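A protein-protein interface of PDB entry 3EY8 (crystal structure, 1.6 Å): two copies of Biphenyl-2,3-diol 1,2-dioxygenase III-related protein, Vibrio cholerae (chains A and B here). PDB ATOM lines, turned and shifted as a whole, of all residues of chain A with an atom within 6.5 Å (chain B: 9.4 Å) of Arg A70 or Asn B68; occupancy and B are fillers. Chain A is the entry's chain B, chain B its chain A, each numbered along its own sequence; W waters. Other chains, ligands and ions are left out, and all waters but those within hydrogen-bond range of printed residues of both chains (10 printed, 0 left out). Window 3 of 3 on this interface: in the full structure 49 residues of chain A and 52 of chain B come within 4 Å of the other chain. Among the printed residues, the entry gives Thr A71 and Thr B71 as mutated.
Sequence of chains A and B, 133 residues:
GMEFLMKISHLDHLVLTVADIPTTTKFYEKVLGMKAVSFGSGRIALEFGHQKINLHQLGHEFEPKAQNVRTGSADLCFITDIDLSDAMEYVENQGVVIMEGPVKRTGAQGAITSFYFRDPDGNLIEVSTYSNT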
ATOM      1  N   THR A  17     -13.374 -33.645  21.166  1.00  0.00           N
ATOM      2  CA  THR A  17     -12.870 -32.885  22.295  1.00  0.00           C
ATOM      3  C   THR A  17     -13.989 -32.795  23.327  1.00  0.00           C
ATOM      4  O   THR A  17     -15.102 -32.362  23.013  1.00  0.00           O
ATOM      5  CB  THR A  17     -12.393 -31.502  21.862  1.00  0.00           C
ATOM      6  OG1 THR A  17     -11.392 -31.655  20.842  1.00  0.00           O
ATOM      7  CG2 THR A  17     -11.791 -30.744  23.056  1.00  0.00           C
ATOM      8  N   LEU A  58     -10.826 -31.019  26.763  1.00  0.00           N
ATOM      9  CA  LEU A  58     -10.776 -29.582  26.547  1.00  0.00           C
ATOM     10  C   LEU A  58      -9.711 -28.981  27.467  1.00  0.00           C
ATOM     11  O   LEU A  58      -9.716 -29.221  28.675  1.00  0.00           O
ATOM     12  CB  LEU A  58     -12.144 -28.962  26.831  1.00  0.00           C
ATOM     13  CG  LEU A  58     -12.313 -27.481  26.494  1.00  0.00           C
ATOM     14  CD1 LEU A  58     -12.159 -27.240  25.005  1.00  0.00           C
ATOM     15  CD2 LEU A  58     -13.674 -27.006  26.976  1.00  0.00           C
ATOM     16  N   ALA A  66      -8.622 -29.777  15.065  1.00  0.00           N
ATOM     17  CA  ALA A  66      -9.608 -28.966  14.350  1.00  0.00           C
ATOM     18  C   ALA A  66      -9.311 -27.477  14.496  1.00  0.00           C
ATOM     19  O   ALA A  66      -8.813 -27.044  15.532  1.00  0.00           O
ATOM     20  CB  ALA A  66     -11.017 -29.275  14.852  1.00  0.00           C
ATOM     21  N   ASN A  68     -11.445 -25.021  14.823  1.00  0.00           N
ATOM     22  CA  ASN A  68     -12.349 -24.471  15.821  1.00  0.00           C
ATOM     23  C   ASN A  68     -12.834 -25.595  16.717  1.00  0.00           C
ATOM     24  O   ASN A  68     -13.925 -26.122  16.527  1.00  0.00           O
ATOM     25  CB  ASN A  68     -13.540 -23.791  15.138  1.00  0.00           C
ATOM     26  CG  ASN A  68     -13.112 -22.687  14.190  1.00  0.00           C
ATOM     27  OD1 ASN A  68     -12.151 -21.959  14.458  1.00  0.00           O
ATOM     28  ND2 ASN A  68     -13.815 -22.561  13.073  1.00  0.00           N
ATOM     29  N   VAL A  69     -11.994 -25.979  17.674  1.00  0.00           N
ATOM     30  CA  VAL A  69     -12.327 -27.059  18.596  1.00  0.00           C
ATOM     31  C   VAL A  69     -13.591 -26.675  19.349  1.00  0.00           C
ATOM     32  O   VAL A  69     -13.739 -25.532  19.776  1.00  0.00           O
ATOM     33  CB  VAL A  69     -11.161 -27.318  19.569  1.00  0.00           C
ATOM     34  CG1 VAL A  69     -11.608 -28.159  20.750  1.00  0.00           C
ATOM     35  CG2 VAL A  69     -10.001 -27.976  18.821  1.00  0.00           C
ATOM     36  N   ARG A  70     -14.516 -27.617  19.484  1.00  0.00           N
ATOM     37  CA  ARG A  70     -15.792 -27.322  20.132  1.00  0.00           C
ATOM     38  C   ARG A  70     -16.387 -28.574  20.754  1.00  0.00           C
ATOM     39  O   ARG A  70     -16.663 -29.556  20.053  1.00  0.00           O
ATOM     40  CB  ARG A  70     -16.778 -26.724  19.126  1.00  0.00           C
ATOM     41  CG  ARG A  70     -18.049 -26.166  19.754  1.00  0.00           C
ATOM     42  CD  ARG A  70     -17.752 -24.863  20.495  1.00  0.00           C
ATOM     43  NE  ARG A  70     -18.968 -24.232  21.008  1.00  0.00           N
ATOM     44  CZ  ARG A  70     -19.401 -24.359  22.259  1.00  0.00           C
ATOM     45  NH1 ARG A  70     -18.718 -25.094  23.128  1.00  0.00           N
ATOM     46  NH2 ARG A  70     -20.515 -23.752  22.642  1.00  0.00           N
ATOM     47  N   THR A  71     -16.591 -28.554  22.068  1.00  0.00           N
ATOM     48  CA  THR A  71     -17.279 -29.664  22.711  1.00  0.00           C
ATOM     49  C   THR A  71     -18.732 -29.695  22.229  1.00  0.00           C
ATOM     50  O   THR A  71     -19.335 -28.653  22.018  1.00  0.00           O
ATOM     51  CB  THR A  71     -17.238 -29.580  24.255  1.00  0.00           C
ATOM     52  OG1 THR A  71     -17.933 -28.407  24.696  1.00  0.00           O
ATOM     53  CG2 THR A  71     -15.781 -29.553  24.762  1.00  0.00           C
ATOM     54  N   GLY A  72     -19.289 -30.888  22.043  1.00  0.00           N
ATOM     55  CA  GLY A  72     -20.673 -31.010  21.615  1.00  0.00           C
ATOM     56  C   GLY A  72     -20.970 -30.655  20.164  1.00  0.00           C
ATOM     57  O   GLY A  72     -22.123 -30.408  19.813  1.00  0.00           O
ATOM     58  N   SER A  73     -19.945 -30.656  19.314  1.00  0.00           N
ATOM     59  CA  SER A  73     -20.089 -30.228  17.919  1.00  0.00           C
ATOM     60  C   SER A  73     -20.187 -31.382  16.931  1.00  0.00           C
ATOM     61  O   SER A  73     -20.250 -31.154  15.724  1.00  0.00           O
ATOM     62  CB  SER A  73     -18.908 -29.336  17.517  1.00  0.00           C
ATOM     63  OG  SER A  73     -17.676 -30.032  17.677  1.00  0.00           O
ATOM     64  N   ALA A  74     -20.171 -32.609  17.440  1.00  0.00           N
ATOM     65  CA  ALA A  74     -20.202 -33.798  16.587  1.00  0.00           C
ATOM     66  C   ALA A  74     -21.608 -34.358  16.422  1.00  0.00           C
ATOM     67  O   ALA A  74     -22.475 -34.169  17.273  1.00  0.00           O
ATOM     68  CB  ALA A  74     -19.263 -34.863  17.129  1.00  0.00           C
ATOM     69  N   ARG A 118     -28.258 -37.762  23.092  1.00  0.00           N
ATOM     70  CA  ARG A 118     -27.042 -36.959  23.200  1.00  0.00           C
ATOM     71  C   ARG A 118     -26.054 -37.546  24.185  1.00  0.00           C
ATOM     72  O   ARG A 118     -26.443 -38.160  25.192  1.00  0.00           O
ATOM     73  CB  ARG A 118     -27.376 -35.519  23.606  1.00  0.00           C
ATOM     74  CG  ARG A 118     -28.145 -34.783  22.533  1.00  0.00           C
ATOM     75  CD  ARG A 118     -28.341 -33.316  22.822  1.00  0.00           C
ATOM     76  NE  ARG A 118     -29.268 -32.758  21.841  1.00  0.00           N
ATOM     77  CZ  ARG A 118     -28.920 -32.396  20.610  1.00  0.00           C
ATOM     78  NH1 ARG A 118     -27.661 -32.522  20.210  1.00  0.00           N
ATOM     79  NH2 ARG A 118     -29.828 -31.906  19.775  1.00  0.00           N
ATOM     80  N   ASP A 121     -21.454 -34.358  26.362  1.00  0.00           N
ATOM     81  CA  ASP A 121     -21.083 -33.028  25.859  1.00  0.00           C
ATOM     82  C   ASP A 121     -22.126 -32.432  24.909  1.00  0.00           C
ATOM     83  O   ASP A 121     -21.967 -31.306  24.422  1.00  0.00           O
ATOM     84  CB  ASP A 121     -19.719 -33.071  25.156  1.00  0.00           C
ATOM     85  CG  ASP A 121     -18.566 -33.326  26.122  1.00  0.00           C
ATOM     86  OD1 ASP A 121     -18.311 -34.506  26.447  1.00  0.00           O
ATOM     87  OD2 ASP A 121     -17.912 -32.347  26.534  1.00  0.00           O
ATOM     88  N   GLY A 122     -23.190 -33.181  24.642  1.00  0.00           N
ATOM     89  CA  GLY A 122     -24.233 -32.707  23.750  1.00  0.00           C
ATOM     90  C   GLY A 122     -24.040 -33.125  22.304  1.00  0.00           C
ATOM     91  O   GLY A 122     -24.822 -32.734  21.442  1.00  0.00           O
ATOM     92  N   ASN A 123     -23.000 -33.907  22.025  1.00  0.00           N
ATOM     93  CA  ASN A 123     -22.870 -34.489  20.688  1.00  0.00           C
ATOM     94  C   ASN A 123     -24.129 -35.282  20.360  1.00  0.00           C
ATOM     95  O   ASN A 123     -24.696 -35.934  21.237  1.00  0.00           O
ATOM     96  CB  ASN A 123     -21.635 -35.386  20.608  1.00  0.00           C
ATOM     97  CG  ASN A 123     -20.344 -34.607  20.790  1.00  0.00           C
ATOM     98  OD1 ASN A 123     -20.123 -33.608  20.114  1.00  0.00           O
ATOM     99  ND2 ASN A 123     -19.481 -35.067  21.700  1.00  0.00           N
ATOM    100  N   VAL B  15     -22.096 -35.860  10.330  1.00  0.00           N
ATOM    101  CA  VAL B  15     -22.547 -34.611   9.727  1.00  0.00           C
ATOM    102  C   VAL B  15     -21.518 -33.509   9.948  1.00  0.00           C
ATOM    103  O   VAL B  15     -21.116 -33.251  11.088  1.00  0.00           O
ATOM    104  CB  VAL B  15     -23.884 -34.141  10.334  1.00  0.00           C
ATOM    105  CG1 VAL B  15     -24.255 -32.772   9.808  1.00  0.00           C
ATOM    106  CG2 VAL B  15     -24.999 -35.160  10.054  1.00  0.00           C
ATOM    107  N   THR B  17     -21.087 -29.424   9.538  1.00  0.00           N
ATOM    108  CA  THR B  17     -21.760 -28.165   9.259  1.00  0.00           C
ATOM    109  C   THR B  17     -20.748 -27.229   8.640  1.00  0.00           C
ATOM    110  O   THR B  17     -19.692 -26.982   9.220  1.00  0.00           O
ATOM    111  CB  THR B  17     -22.350 -27.564  10.535  1.00  0.00           C
ATOM    112  OG1 THR B  17     -23.354 -28.456  11.031  1.00  0.00           O
ATOM    113  CG2 THR B  17     -22.989 -26.199  10.247  1.00  0.00           C
ATOM    114  N   LEU B  58     -24.325 -23.976   7.439  1.00  0.00           N
ATOM    115  CA  LEU B  58     -24.483 -23.140   8.629  1.00  0.00           C
ATOM    116  C   LEU B  58     -25.624 -22.153   8.429  1.00  0.00           C
ATOM    117  O   LEU B  58     -25.672 -21.439   7.430  1.00  0.00           O
ATOM    118  CB  LEU B  58     -23.198 -22.363   8.926  1.00  0.00           C
ATOM    119  CG  LEU B  58     -23.137 -21.524  10.209  1.00  0.00           C
ATOM    120  CD1 LEU B  58     -23.085 -22.416  11.453  1.00  0.00           C
ATOM    121  CD2 LEU B  58     -21.946 -20.577  10.190  1.00  0.00           C
ATOM    122  N   LYS B  65     -29.603 -31.668  15.534  1.00  0.00           N
ATOM    123  CA  LYS B  65     -28.197 -31.555  15.161  1.00  0.00           C
ATOM    124  C   LYS B  65     -27.328 -31.539  16.412  1.00  0.00           C
ATOM    125  O   LYS B  65     -27.821 -31.735  17.522  1.00  0.00           O
ATOM    126  CB  LYS B  65     -27.971 -30.297  14.326  1.00  0.00           C
ATOM    127  CG  LYS B  65     -28.419 -29.025  15.010  1.00  0.00           C
ATOM    128  CD  LYS B  65     -28.640 -27.909  13.991  1.00  0.00           C
ATOM    129  CE  LYS B  65     -29.134 -26.644  14.674  1.00  0.00           C
ATOM    130  NZ  LYS B  65     -29.496 -25.591  13.690  1.00  0.00           N
ATOM    131  N   ALA B  66     -26.030 -31.334  16.234  1.00  0.00           N
ATOM    132  CA  ALA B  66     -25.127 -31.245  17.370  1.00  0.00           C
ATOM    133  C   ALA B  66     -25.602 -30.132  18.306  1.00  0.00           C
ATOM    134  O   ALA B  66     -26.189 -29.142  17.859  1.00  0.00           O
ATOM    135  CB  ALA B  66     -23.711 -30.967  16.889  1.00  0.00           C
ATOM    136  N   GLN B  67     -25.345 -30.283  19.596  1.00  0.00           N
ATOM    137  CA  GLN B  67     -25.741 -29.255  20.555  1.00  0.00           C
ATOM    138  C   GLN B  67     -25.067 -27.927  20.220  1.00  0.00           C
ATOM    139  O   GLN B  67     -25.699 -26.860  20.249  1.00  0.00           O
ATOM    140  CB  GLN B  67     -25.364 -29.682  21.970  1.00  0.00           C
ATOM    141  CG  GLN B  67     -25.648 -28.616  23.017  1.00  0.00           C
ATOM    142  CD  GLN B  67     -25.468 -29.135  24.425  1.00  0.00           C
ATOM    143  OE1 GLN B  67     -26.241 -29.969  24.890  1.00  0.00           O
ATOM    144  NE2 GLN B  67     -24.444 -28.643  25.114  1.00  0.00           N
ATOM    145  N   ASN B  68     -23.777 -28.003  19.912  1.00  0.00           N
ATOM    146  CA  ASN B  68     -22.976 -26.837  19.562  1.00  0.00           C
ATOM    147  C   ASN B  68     -22.413 -26.949  18.159  1.00  0.00           C
ATOM    148  O   ASN B  68     -21.241 -27.287  17.973  1.00  0.00           O
ATOM    149  CB  ASN B  68     -21.851 -26.660  20.574  1.00  0.00           C
ATOM    150  CG  ASN B  68     -22.374 -26.528  21.983  1.00  0.00           C
ATOM    151  OD1 ASN B  68     -23.355 -25.829  22.218  1.00  0.00           O
ATOM    152  ND2 ASN B  68     -21.738 -27.206  22.921  1.00  0.00           N
ATOM    153  N   VAL B  69     -23.260 -26.680  17.172  1.00  0.00           N
ATOM    154  CA  VAL B  69     -22.836 -26.703  15.776  1.00  0.00           C
ATOM    155  C   VAL B  69     -21.702 -25.713  15.582  1.00  0.00           C
ATOM    156  O   VAL B  69     -21.736 -24.599  16.112  1.00  0.00           O
ATOM    157  CB  VAL B  69     -24.016 -26.359  14.850  1.00  0.00           C
ATOM    158  CG1 VAL B  69     -23.528 -26.017  13.456  1.00  0.00           C
ATOM    159  CG2 VAL B  69     -25.025 -27.524  14.828  1.00  0.00           C
ATOM    160  N   ARG B  70     -20.676 -26.132  14.853  1.00  0.00           N
ATOM    161  CA  ARG B  70     -19.516 -25.277  14.641  1.00  0.00           C
ATOM    162  C   ARG B  70     -18.766 -25.672  13.380  1.00  0.00           C
ATOM    163  O   ARG B  70     -18.336 -26.811  13.238  1.00  0.00           O
ATOM    164  CB  ARG B  70     -18.581 -25.346  15.848  1.00  0.00           C
ATOM    165  CG  ARG B  70     -17.403 -24.376  15.774  1.00  0.00           C
ATOM    166  CD  ARG B  70     -17.832 -22.957  16.148  1.00  0.00           C
ATOM    167  NE  ARG B  70     -16.686 -22.054  16.254  1.00  0.00           N
ATOM    168  CZ  ARG B  70     -16.237 -21.302  15.255  1.00  0.00           C
ATOM    169  NH1 ARG B  70     -16.835 -21.341  14.073  1.00  0.00           N
ATOM    170  NH2 ARG B  70     -15.186 -20.509  15.440  1.00  0.00           N
ATOM    171  N   THR B  71     -18.618 -24.732  12.456  1.00  0.00           N
ATOM    172  CA  THR B  71     -17.834 -24.993  11.252  1.00  0.00           C
ATOM    173  C   THR B  71     -16.377 -25.191  11.666  1.00  0.00           C
ATOM    174  O   THR B  71     -15.893 -24.541  12.597  1.00  0.00           O
ATOM    175  CB  THR B  71     -17.927 -23.820  10.249  1.00  0.00           C
ATOM    176  OG1 THR B  71     -17.502 -22.612  10.893  1.00  0.00           O
ATOM    177  CG2 THR B  71     -19.362 -23.641   9.765  1.00  0.00           C
ATOM    178  N   GLY B  72     -15.672 -26.089  10.986  1.00  0.00           N
ATOM    179  CA  GLY B  72     -14.255 -26.292  11.243  1.00  0.00           C
ATOM    180  C   GLY B  72     -13.922 -26.983  12.559  1.00  0.00           C
ATOM    181  O   GLY B  72     -12.795 -26.875  13.054  1.00  0.00           O
ATOM    182  N   SER B  73     -14.889 -27.710  13.114  1.00  0.00           N
ATOM    183  CA  SER B  73     -14.742 -28.369  14.414  1.00  0.00           C
ATOM    184  C   SER B  73     -14.462 -29.862  14.314  1.00  0.00           C
ATOM    185  O   SER B  73     -14.416 -30.547  15.338  1.00  0.00           O
ATOM    186  CB  SER B  73     -16.010 -28.175  15.248  1.00  0.00           C
ATOM    187  OG  SER B  73     -17.135 -28.759  14.597  1.00  0.00           O
ATOM    188  N   ALA B  74     -14.302 -30.373  13.095  1.00  0.00           N
ATOM    189  CA  ALA B  74     -14.056 -31.801  12.912  1.00  0.00           C
ATOM    190  C   ALA B  74     -12.583 -32.125  12.681  1.00  0.00           C
ATOM    191  O   ALA B  74     -11.790 -31.292  12.227  1.00  0.00           O
ATOM    192  CB  ALA B  74     -14.910 -32.364  11.768  1.00  0.00           C
ATOM    193  N   ASP B  75     -12.236 -33.366  12.979  1.00  0.00           N
ATOM    194  CA  ASP B  75     -10.847 -33.805  13.022  1.00  0.00           C
ATOM    195  C   ASP B  75     -10.913 -35.260  12.602  1.00  0.00           C
ATOM    196  O   ASP B  75     -11.260 -36.125  13.400  1.00  0.00           O
ATOM    197  CB  ASP B  75     -10.331 -33.621  14.455  1.00  0.00           C
ATOM    198  CG  ASP B  75      -8.862 -33.973  14.624  1.00  0.00           C
ATOM    199  OD1 ASP B  75      -8.309 -34.731  13.793  1.00  0.00           O
ATOM    200  OD2 ASP B  75      -8.264 -33.498  15.624  1.00  0.00           O
ATOM    201  N   ASN B 123     -11.663 -27.770   9.014  1.00  0.00           N
ATOM    202  CA  ASN B 123     -11.638 -29.111   9.575  1.00  0.00           C
ATOM    203  C   ASN B 123     -10.281 -29.736   9.291  1.00  0.00           C
ATOM    204  O   ASN B 123      -9.697 -29.504   8.227  1.00  0.00           O
ATOM    205  CB  ASN B 123     -12.750 -29.969   8.979  1.00  0.00           C
ATOM    206  CG  ASN B 123     -14.125 -29.433   9.295  1.00  0.00           C
ATOM    207  OD1 ASN B 123     -14.471 -29.220  10.463  1.00  0.00           O
ATOM    208  ND2 ASN B 123     -14.927 -29.215   8.258  1.00  0.00           N
HETATM  209  O   HOH W   1      -9.643 -31.636  17.167  1.00  0.00           O
HETATM  210  O   HOH W   2     -16.345 -32.306  16.691  1.00  0.00           O
HETATM  211  O   HOH W   3     -13.963 -30.082  18.068  1.00  0.00           O
HETATM  212  O   HOH W   4     -30.664 -29.928  17.604  1.00  0.00           O
HETATM  213  O   HOH W   5     -28.514 -29.782  23.290  1.00  0.00           O
HETATM  214  O   HOH W   6     -20.575 -29.175  25.272  1.00  0.00           O
HETATM  215  O   HOH W   7     -14.775 -22.277   9.957  1.00  0.00           O
HETATM  216  O   HOH W   8     -18.143 -31.240  13.552  1.00  0.00           O
HETATM  217  O   HOH W   9     -20.832 -23.473  18.529  1.00  0.00           O
HETATM  218  O   HOH W  10     -20.862 -29.017  14.134  1.00  0.00           O
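Water W6 lies within hydrogen-bond range of the backbone carbonyl oxygen of Asp A121 (2.7 Å), the side-chain hydroxyl of Thr A71 (2.8 Å) and the side-chain amide nitrogen of Asn B68 (3.3 Å). Water W1 bridges the side-chain carboxylate of Asp B75 (2.8 Å) and the backbone NH of Ala A66 (3.0 Å). Water W3 lies within hydrogen-bond range of O of Ser B73 (2.8 Å) and N of Arg A70 (2.9 Å). Water W9 bridges the backbone carbonyl oxygen of Val B69 (2.8 Å) and the guanidinium group of Arg A70 (3.2 Å). Water W7 lies within hydrogen-bond range of the side-chain hydroxyl (OG1) of Thr B71 (2.9 Å) and the side-chain amide nitrogen (ND2) of Asn A68 (3.3 Å). Water W4 bridges the backbone NH of Lys B65 (2.9 Å) and the guanidinium group of Arg A118 (3.1 Å).
The backbone carbonyl oxygen (O) of Lys B65 is in hydrogen-bond range of the guanidinium group (NH1) of Arg A118. The backbone carbonyl oxygen (O) of Gly A72 sits at hydrogen-bond distance from the backbone NH (N) of Gln B67, 3.2 Å away. The backbone NH of Gln B67 lies within hydrogen-bond range of the backbone carbonyl oxygen of Gly A122 (3.1 Å). O of Thr A71 sits at hydrogen-bond distance from ND2 of Asn B68, 2.9 Å away. The backbone carbonyl oxygen of Gly A72 sits at hydrogen-bond distance from the backbone NH of Asn B68, at 2.9 Å. The side-chain amide nitrogen (ND2) of Asn A68 lies close to the guanidinium group (NH1) of Arg B70, at 3.4 Å. O of Thr B71 is in hydrogen-bond range of ND2 of Asn A68 (2.9 Å). The backbone NH of Asn A68 sits at hydrogen-bond distance from the backbone carbonyl oxygen of Gly B72 (2.9 Å). OG of Ser B73 lies within hydrogen-bond range of OG of Ser A73, at 3.4 Å. The backbone NH of Gln B67 sits close to the guanidinium group of Arg A118.
Among the printed residues, merely in contact across the chains: Ser A73 with Asn B68 (3.1 Å), Asn A68 with Ser B73 (3.2 Å), Gly A72 with Ala B66 (3.4 Å), Ala A66 with Ala B74 (3.4 Å), Arg A70 with Asn B68 (3.4 Å), Ala A74 with Ala B66 (3.5 Å), Ala A66 with Gly B72 (3.5 Å), Ala A66 with Ser B73 (3.5 Å), Ser A73 with Ala B66 (3.5 Å), Arg A118 with Ala B66 (3.7 Å), Asp A121 with Gln B67 (3.7 Å), Ala A66 with Asp B75 (3.8 Å) and Arg A70 with Arg B70 (3.99 Å).
Ala A66 touches Ala B74, and with the chains exchanged Ala A74 touches Ala B66. Asn A68 touches Arg B70, and with the chains exchanged Arg A70 touches Asn B68. Asn A68 touches Ser B73, and with the chains exchanged Ser A73 touches Asn B68. Arg B70 touches its own counterpart, Arg A70. Positions printed for both chains: 17, 58, 66, 68, 69, 70, 71, 72, 73, 74 and 123. Of the 23 pairs that touch across the chains among the printed residues, 16 have their exchanged pair printed and touching as well.
Among the printed residues, no Asp or Glu carboxylate lies within 4 Å of a Lys or Arg side-chain nitrogen of the other chain.
The side-chain hydroxyl of Thr B71 sits at hydrogen-bond distance from the guanidinium group of Arg B70. The backbone carbonyl oxygen of Arg B70 lies within hydrogen-bond range of the side-chain hydroxyl of Ser B73 (2.7 Å). The side-chain amide oxygen (OD1) of Asn B123 sits close to the backbone NH (N) of Gly B72. N of Gly A72 sits close to OD1 of Asn A123 (3.4 Å). The backbone NH (N) of Ser A73 sits at hydrogen-bond distance from the side-chain amide oxygen (OD1) of Asn A123. The side-chain amide oxygen of Asn A123 lies within hydrogen-bond range of the backbone NH of Ala A74 (2.9 Å).
Of the printed residues of chain B, Arg A70 touches Asn B68 (3.4 Å) and Arg B70 (3.99 Å). Of chain A, only Arg A70, Thr A71, Gly A72 and Ser A73 come within 4 Å of Asn B68. Thr A71 touches one residue of chain B. Gly A72 touches just these residues of chain B: Ala B66, Gln B67 and Asn B68. Of chain B, only Ala B66 (3.5 Å), Asn B68 (3.1 Å) and Ser B73 (3.4 Å) come within 4 Å of Ser A73. Printed residues of chain A within 4 Å of Ala B66: Gly A72 (3.4 Å), Ser A73 (3.5 Å), Ala A74 (3.5 Å) and Arg A118 (3.7 Å). Of the printed residues of chain A, Thr B71 touches Asn A68. Of the printed residues of chain B, Ala A66 touches Gly B72 (3.5 Å), Ser B73 (3.5 Å), Ala B74 (3.4 Å) and Asp B75 (3.8 Å). Printed residues of chain A within 4 Å of Arg B70: Asn A68 (3.3 Å) and Arg A70 (3.99 Å). Of the printed residues of chain A, Ala B74 touches Ala A66 (3.4 Å). The nearest printed residue of chain B that does not touch Arg A70 is Ser B73 (4.2 Å). The nearest residue of chain A that does not touch Asn B68 is Asp A121 (4.4 Å).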
